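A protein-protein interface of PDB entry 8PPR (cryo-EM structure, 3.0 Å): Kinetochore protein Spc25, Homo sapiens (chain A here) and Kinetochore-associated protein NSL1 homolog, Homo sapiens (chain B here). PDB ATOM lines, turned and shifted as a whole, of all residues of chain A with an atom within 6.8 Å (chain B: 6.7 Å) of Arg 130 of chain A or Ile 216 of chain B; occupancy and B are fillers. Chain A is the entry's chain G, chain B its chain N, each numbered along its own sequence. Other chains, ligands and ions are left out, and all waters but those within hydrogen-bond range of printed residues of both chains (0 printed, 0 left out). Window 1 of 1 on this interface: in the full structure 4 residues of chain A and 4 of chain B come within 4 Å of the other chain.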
ATOM      1  N   ALA A 125      -2.329 -16.932   9.963  1.00  0.00           N
ATOM      2  CA  ALA A 125      -1.539 -16.054  10.815  1.00  0.00           C
ATOM      3  C   ALA A 125      -2.047 -16.078  12.249  1.00  0.00           C
ATOM      4  O   ALA A 125      -1.256 -16.130  13.193  1.00  0.00           O
ATOM      5  CB  ALA A 125      -1.559 -14.629  10.260  1.00  0.00           C
ATOM      6  N   GLU A 126      -3.368 -16.033  12.435  1.00  0.00           N
ATOM      7  CA  GLU A 126      -3.914 -16.072  13.791  1.00  0.00           C
ATOM      8  C   GLU A 126      -3.600 -17.397  14.474  1.00  0.00           C
ATOM      9  O   GLU A 126      -3.244 -17.428  15.663  1.00  0.00           O
ATOM     10  CB  GLU A 126      -5.420 -15.825  13.760  1.00  0.00           C
ATOM     11  CG  GLU A 126      -5.792 -14.437  13.283  1.00  0.00           C
ATOM     12  CD  GLU A 126      -5.280 -13.354  14.211  1.00  0.00           C
ATOM     13  OE1 GLU A 126      -5.200 -13.603  15.432  1.00  0.00           O
ATOM     14  OE2 GLU A 126      -4.950 -12.256  13.718  1.00  0.00           O
ATOM     15  N   ARG A 127      -3.728 -18.504  13.740  1.00  0.00           N
ATOM     16  CA  ARG A 127      -3.378 -19.801  14.310  1.00  0.00           C
ATOM     17  C   ARG A 127      -1.906 -19.841  14.705  1.00  0.00           C
ATOM     18  O   ARG A 127      -1.549 -20.332  15.785  1.00  0.00           O
ATOM     19  CB  ARG A 127      -3.714 -20.908  13.311  1.00  0.00           C
ATOM     20  CG  ARG A 127      -5.197 -20.995  12.993  1.00  0.00           C
ATOM     21  CD  ARG A 127      -5.470 -21.888  11.798  1.00  0.00           C
ATOM     22  NE  ARG A 127      -4.990 -23.248  12.007  1.00  0.00           N
ATOM     23  CZ  ARG A 127      -4.124 -23.862  11.213  1.00  0.00           C
ATOM     24  NH1 ARG A 127      -3.640 -23.271  10.132  1.00  0.00           N
ATOM     25  NH2 ARG A 127      -3.738 -25.100  11.507  1.00  0.00           N
ATOM     26  N   LEU A 128      -1.039 -19.306  13.844  1.00  0.00           N
ATOM     27  CA  LEU A 128       0.385 -19.260  14.155  1.00  0.00           C
ATOM     28  C   LEU A 128       0.661 -18.378  15.365  1.00  0.00           C
ATOM     29  O   LEU A 128       1.550 -18.679  16.163  1.00  0.00           O
ATOM     30  CB  LEU A 128       1.173 -18.767  12.942  1.00  0.00           C
ATOM     31  CG  LEU A 128       2.646 -18.451  13.202  1.00  0.00           C
ATOM     32  CD1 LEU A 128       3.443 -19.729  13.419  1.00  0.00           C
ATOM     33  CD2 LEU A 128       3.233 -17.633  12.064  1.00  0.00           C
ATOM     34  N   LYS A 129      -0.075 -17.276  15.508  1.00  0.00           N
ATOM     35  CA  LYS A 129       0.105 -16.410  16.670  1.00  0.00           C
ATOM     36  C   LYS A 129      -0.266 -17.135  17.954  1.00  0.00           C
ATOM     37  O   LYS A 129       0.432 -17.023  18.968  1.00  0.00           O
ATOM     38  CB  LYS A 129      -0.725 -15.135  16.517  1.00  0.00           C
ATOM     39  CG  LYS A 129      -0.309 -14.261  15.355  1.00  0.00           C
ATOM     40  CD  LYS A 129      -1.350 -13.197  15.070  1.00  0.00           C
ATOM     41  CE  LYS A 129      -1.015 -12.437  13.800  1.00  0.00           C
ATOM     42  NZ  LYS A 129       0.323 -11.792  13.883  1.00  0.00           N
ATOM     43  N   ARG A 130      -1.373 -17.880  17.933  1.00  0.00           N
ATOM     44  CA  ARG A 130      -1.741 -18.663  19.109  1.00  0.00           C
ATOM     45  C   ARG A 130      -0.665 -19.693  19.438  1.00  0.00           C
ATOM     46  O   ARG A 130      -0.257 -19.842  20.602  1.00  0.00           O
ATOM     47  CB  ARG A 130      -3.085 -19.351  18.878  1.00  0.00           C
ATOM     48  CG  ARG A 130      -4.290 -18.442  19.031  1.00  0.00           C
ATOM     49  CD  ARG A 130      -5.556 -19.255  19.227  1.00  0.00           C
ATOM     50  NE  ARG A 130      -6.735 -18.411  19.378  1.00  0.00           N
ATOM     51  CZ  ARG A 130      -7.779 -18.436  18.562  1.00  0.00           C
ATOM     52  NH1 ARG A 130      -7.824 -19.253  17.522  1.00  0.00           N
ATOM     53  NH2 ARG A 130      -8.805 -17.623  18.797  1.00  0.00           N
ATOM     54  N   LEU A 131      -0.182 -20.401  18.415  1.00  0.00           N
ATOM     55  CA  LEU A 131       0.854 -21.405  18.628  1.00  0.00           C
ATOM     56  C   LEU A 131       2.135 -20.774  19.159  1.00  0.00           C
ATOM     57  O   LEU A 131       2.801 -21.339  20.034  1.00  0.00           O
ATOM     58  CB  LEU A 131       1.122 -22.151  17.324  1.00  0.00           C
ATOM     59  CG  LEU A 131      -0.033 -23.003  16.796  1.00  0.00           C
ATOM     60  CD1 LEU A 131       0.260 -23.485  15.386  1.00  0.00           C
ATOM     61  CD2 LEU A 131      -0.298 -24.179  17.721  1.00  0.00           C
ATOM     62  N   GLN A 132       2.495 -19.602  18.636  1.00  0.00           N
ATOM     63  CA  GLN A 132       3.691 -18.909  19.091  1.00  0.00           C
ATOM     64  C   GLN A 132       3.537 -18.429  20.524  1.00  0.00           C
ATOM     65  O   GLN A 132       4.499 -18.457  21.293  1.00  0.00           O
ATOM     66  CB  GLN A 132       4.004 -17.737  18.163  1.00  0.00           C
ATOM     67  CG  GLN A 132       5.444 -17.272  18.242  1.00  0.00           C
ATOM     68  CD  GLN A 132       6.430 -18.381  17.934  1.00  0.00           C
ATOM     69  OE1 GLN A 132       6.172 -19.241  17.091  1.00  0.00           O
ATOM     70  NE2 GLN A 132       7.563 -18.372  18.623  1.00  0.00           N
ATOM     71  N   LYS A 133       2.340 -17.979  20.898  1.00  0.00           N
ATOM     72  CA  LYS A 133       2.095 -17.614  22.288  1.00  0.00           C
ATOM     73  C   LYS A 133       2.309 -18.809  23.205  1.00  0.00           C
ATOM     74  O   LYS A 133       2.966 -18.700  24.249  1.00  0.00           O
ATOM     75  CB  LYS A 133       0.680 -17.060  22.441  1.00  0.00           C
ATOM     76  CG  LYS A 133       0.285 -16.774  23.876  1.00  0.00           C
ATOM     77  CD  LYS A 133       1.182 -15.723  24.501  1.00  0.00           C
ATOM     78  CE  LYS A 133       1.085 -15.761  26.017  1.00  0.00           C
ATOM     79  NZ  LYS A 133       1.408 -14.445  26.631  1.00  0.00           N
ATOM     80  N   SER A 134       1.772 -19.969  22.819  1.00  0.00           N
ATOM     81  CA  SER A 134       1.951 -21.165  23.639  1.00  0.00           C
ATOM     82  C   SER A 134       3.425 -21.552  23.741  1.00  0.00           C
ATOM     83  O   SER A 134       3.935 -21.838  24.835  1.00  0.00           O
ATOM     84  CB  SER A 134       1.130 -22.318  23.064  1.00  0.00           C
ATOM     85  OG  SER A 134       1.554 -23.559  23.600  1.00  0.00           O
ATOM     86  N   ALA A 135       4.126 -21.560  22.606  1.00  0.00           N
ATOM     87  CA  ALA A 135       5.533 -21.948  22.603  1.00  0.00           C
ATOM     88  C   ALA A 135       6.376 -20.965  23.403  1.00  0.00           C
ATOM     89  O   ALA A 135       7.316 -21.363  24.098  1.00  0.00           O
ATOM     90  CB  ALA A 135       6.046 -22.052  21.168  1.00  0.00           C
ATOM     91  N   LEU B 213     -10.722 -26.980  27.301  1.00  0.00           N
ATOM     92  CA  LEU B 213     -11.613 -26.155  26.496  1.00  0.00           C
ATOM     93  C   LEU B 213     -10.931 -24.914  25.935  1.00  0.00           C
ATOM     94  O   LEU B 213     -11.533 -24.219  25.111  1.00  0.00           O
ATOM     95  CB  LEU B 213     -12.830 -25.737  27.322  1.00  0.00           C
ATOM     96  CG  LEU B 213     -13.793 -26.856  27.726  1.00  0.00           C
ATOM     97  CD1 LEU B 213     -15.171 -26.292  28.027  1.00  0.00           C
ATOM     98  CD2 LEU B 213     -13.870 -27.926  26.645  1.00  0.00           C
ATOM     99  N   GLN B 214      -9.705 -24.622  26.357  1.00  0.00           N
ATOM    100  CA  GLN B 214      -9.020 -23.425  25.894  1.00  0.00           C
ATOM    101  C   GLN B 214      -8.645 -23.557  24.423  1.00  0.00           C
ATOM    102  O   GLN B 214      -8.171 -24.606  23.977  1.00  0.00           O
ATOM    103  CB  GLN B 214      -7.775 -23.176  26.743  1.00  0.00           C
ATOM    104  CG  GLN B 214      -8.077 -23.090  28.229  1.00  0.00           C
ATOM    105  CD  GLN B 214      -6.940 -22.488  29.025  1.00  0.00           C
ATOM    106  OE1 GLN B 214      -5.795 -22.485  28.585  1.00  0.00           O
ATOM    107  NE2 GLN B 214      -7.256 -21.970  30.205  1.00  0.00           N
ATOM    108  N   ARG B 215      -8.860 -22.477  23.668  1.00  0.00           N
ATOM    109  CA  ARG B 215      -8.609 -22.511  22.231  1.00  0.00           C
ATOM    110  C   ARG B 215      -7.138 -22.752  21.926  1.00  0.00           C
ATOM    111  O   ARG B 215      -6.805 -23.509  21.007  1.00  0.00           O
ATOM    112  CB  ARG B 215      -9.073 -21.210  21.583  1.00  0.00           C
ATOM    113  CG  ARG B 215      -9.040 -21.244  20.067  1.00  0.00           C
ATOM    114  CD  ARG B 215     -10.248 -21.974  19.510  1.00  0.00           C
ATOM    115  NE  ARG B 215     -11.480 -21.591  20.190  1.00  0.00           N
ATOM    116  CZ  ARG B 215     -12.065 -20.405  20.079  1.00  0.00           C
ATOM    117  NH1 ARG B 215     -11.570 -19.458  19.297  1.00  0.00           N
ATOM    118  NH2 ARG B 215     -13.179 -20.164  20.766  1.00  0.00           N
ATOM    119  N   ILE B 216      -6.244 -22.102  22.673  1.00  0.00           N
ATOM    120  CA  ILE B 216      -4.814 -22.303  22.459  1.00  0.00           C
ATOM    121  C   ILE B 216      -4.444 -23.755  22.717  1.00  0.00           C
ATOM    122  O   ILE B 216      -3.713 -24.375  21.935  1.00  0.00           O
ATOM    123  CB  ILE B 216      -4.006 -21.345  23.351  1.00  0.00           C
ATOM    124  CG1 ILE B 216      -4.429 -19.900  23.093  1.00  0.00           C
ATOM    125  CG2 ILE B 216      -2.517 -21.524  23.107  1.00  0.00           C
ATOM    126  CD1 ILE B 216      -3.615 -18.882  23.858  1.00  0.00           C
ATOM    127  N   HIS B 217      -4.955 -24.322  23.811  1.00  0.00           N
ATOM    128  CA  HIS B 217      -4.704 -25.726  24.108  1.00  0.00           C
ATOM    129  C   HIS B 217      -5.259 -26.625  23.012  1.00  0.00           C
ATOM    130  O   HIS B 217      -4.610 -27.596  22.605  1.00  0.00           O
ATOM    131  CB  HIS B 217      -5.317 -26.083  25.462  1.00  0.00           C
ATOM    132  CG  HIS B 217      -5.231 -27.537  25.804  1.00  0.00           C
ATOM    133  ND1 HIS B 217      -6.090 -28.479  25.277  1.00  0.00           N
ATOM    134  CD2 HIS B 217      -4.394 -28.211  26.627  1.00  0.00           C
ATOM    135  CE1 HIS B 217      -5.781 -29.670  25.755  1.00  0.00           C
ATOM    136  NE2 HIS B 217      -4.755 -29.536  26.577  1.00  0.00           N
ATOM    137  N   GLN B 218      -6.460 -26.314  22.521  1.00  0.00           N
ATOM    138  CA  GLN B 218      -7.067 -27.128  21.474  1.00  0.00           C
ATOM    139  C   GLN B 218      -6.230 -27.105  20.203  1.00  0.00           C
ATOM    140  O   GLN B 218      -5.994 -28.149  19.585  1.00  0.00           O
ATOM    141  CB  GLN B 218      -8.482 -26.629  21.192  1.00  0.00           C
ATOM    142  CG  GLN B 218      -9.474 -26.946  22.292  1.00  0.00           C
ATOM    143  CD  GLN B 218     -10.908 -26.789  21.840  1.00  0.00           C
ATOM    144  OE1 GLN B 218     -11.201 -26.822  20.645  1.00  0.00           O
ATOM    145  NE2 GLN B 218     -11.813 -26.610  22.794  1.00  0.00           N
ATOM    146  N   GLU B 219      -5.771 -25.919  19.800  1.00  0.00           N
ATOM    147  CA  GLU B 219      -4.956 -25.813  18.596  1.00  0.00           C
ATOM    148  C   GLU B 219      -3.621 -26.522  18.771  1.00  0.00           C
ATOM    149  O   GLU B 219      -3.154 -27.215  17.859  1.00  0.00           O
ATOM    150  CB  GLU B 219      -4.737 -24.345  18.240  1.00  0.00           C
ATOM    151  CG  GLU B 219      -5.976 -23.645  17.713  1.00  0.00           C
ATOM    152  CD  GLU B 219      -5.719 -22.191  17.381  1.00  0.00           C
ATOM    153  OE1 GLU B 219      -4.540 -21.782  17.379  1.00  0.00           O
ATOM    154  OE2 GLU B 219      -6.695 -21.456  17.124  1.00  0.00           O
ATOM    155  N   VAL B 220      -2.992 -26.360  19.935  1.00  0.00           N
ATOM    156  CA  VAL B 220      -1.714 -27.016  20.185  1.00  0.00           C
ATOM    157  C   VAL B 220      -1.883 -28.529  20.208  1.00  0.00           C
ATOM    158  O   VAL B 220      -1.095 -29.265  19.603  1.00  0.00           O
ATOM    159  CB  VAL B 220      -1.098 -26.496  21.495  1.00  0.00           C
ATOM    160  CG1 VAL B 220       0.082 -27.359  21.902  1.00  0.00           C
ATOM    161  CG2 VAL B 220      -0.669 -25.049  21.336  1.00  0.00           C
ATOM    162  N   PHE B 221      -2.919 -29.016  20.889  1.00  0.00           N
ATOM    163  CA  PHE B 221      -3.126 -30.444  21.073  1.00  0.00           C
ATOM    164  C   PHE B 221      -4.057 -31.037  20.026  1.00  0.00           C
ATOM    165  O   PHE B 221      -4.664 -32.084  20.267  1.00  0.00           O
ATOM    166  CB  PHE B 221      -3.658 -30.718  22.478  1.00  0.00           C
ATOM    167  CG  PHE B 221      -2.627 -30.542  23.552  1.00  0.00           C
ATOM    168  CD1 PHE B 221      -1.813 -31.594  23.926  1.00  0.00           C
ATOM    169  CD2 PHE B 221      -2.461 -29.317  24.173  1.00  0.00           C
ATOM    170  CE1 PHE B 221      -0.858 -31.434  24.910  1.00  0.00           C
ATOM    171  CE2 PHE B 221      -1.508 -29.149  25.158  1.00  0.00           C
ATOM    172  CZ  PHE B 221      -0.704 -30.209  25.528  1.00  0.00           C
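The guanidinium group (NH1) of Arg 130 of chain A lies within salt-bridge range of the side-chain carboxylate (OE2) of Glu 219 of chain B (2.5 Å). NH2 of Arg 130 of chain A sits close to NH1 of Arg 215 of chain B (3.4 Å).
Among the printed residues, merely in contact across the chains: Arg 127 of chain A with Glu 219 of chain B, Arg 130 of chain A with Ile 216 of chain B, Leu 131 of chain A with Val 220 of chain B, Ser 134 of chain A with Ile 216 of chain B and Ser 134 of chain A with Val 220 of chain B.
Of the printed residues of chain B, Arg 130 of chain A touches Arg 215 (3.4 Å), Ile 216 (3.8 Å) and Glu 219 (2.5 Å). Of the printed residues of chain A, Arg 215 of chain B touches Arg 130. Ile 216 of chain B touches two residues of chain A. His 217 of chain B touches none of the printed residues of chain A. Of the printed residues of chain A, Glu 219 of chain B touches Arg 127 (3.7 Å) and Arg 130 (2.5 Å). Of the printed residues of chain A, Val 220 of chain B touches Leu 131 and Ser 134. The nearest residue of chain A that does not touch Ile 216 of chain B is Lys 133 of chain A (4.4 Å). The nearest printed residue of chain A that does not touch Glu 219 of chain B is Leu 131 of chain A (4.2 Å).
Hydrophobic or aromatic side chains of chain A within 4 Å of the printed part of chain B: Leu 131. Along chain A the printed residues that touch a printed residue of chain B span positions 127 to 134. Of the 9 printed residues of chain B, 4 touch a printed residue of chain A. Printed residues of chain B that touch a printed residue of chain A: Arg 215, Ile 216, Glu 219 and Val 220. Among the printed residues, 7 pairs touch across the chains.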
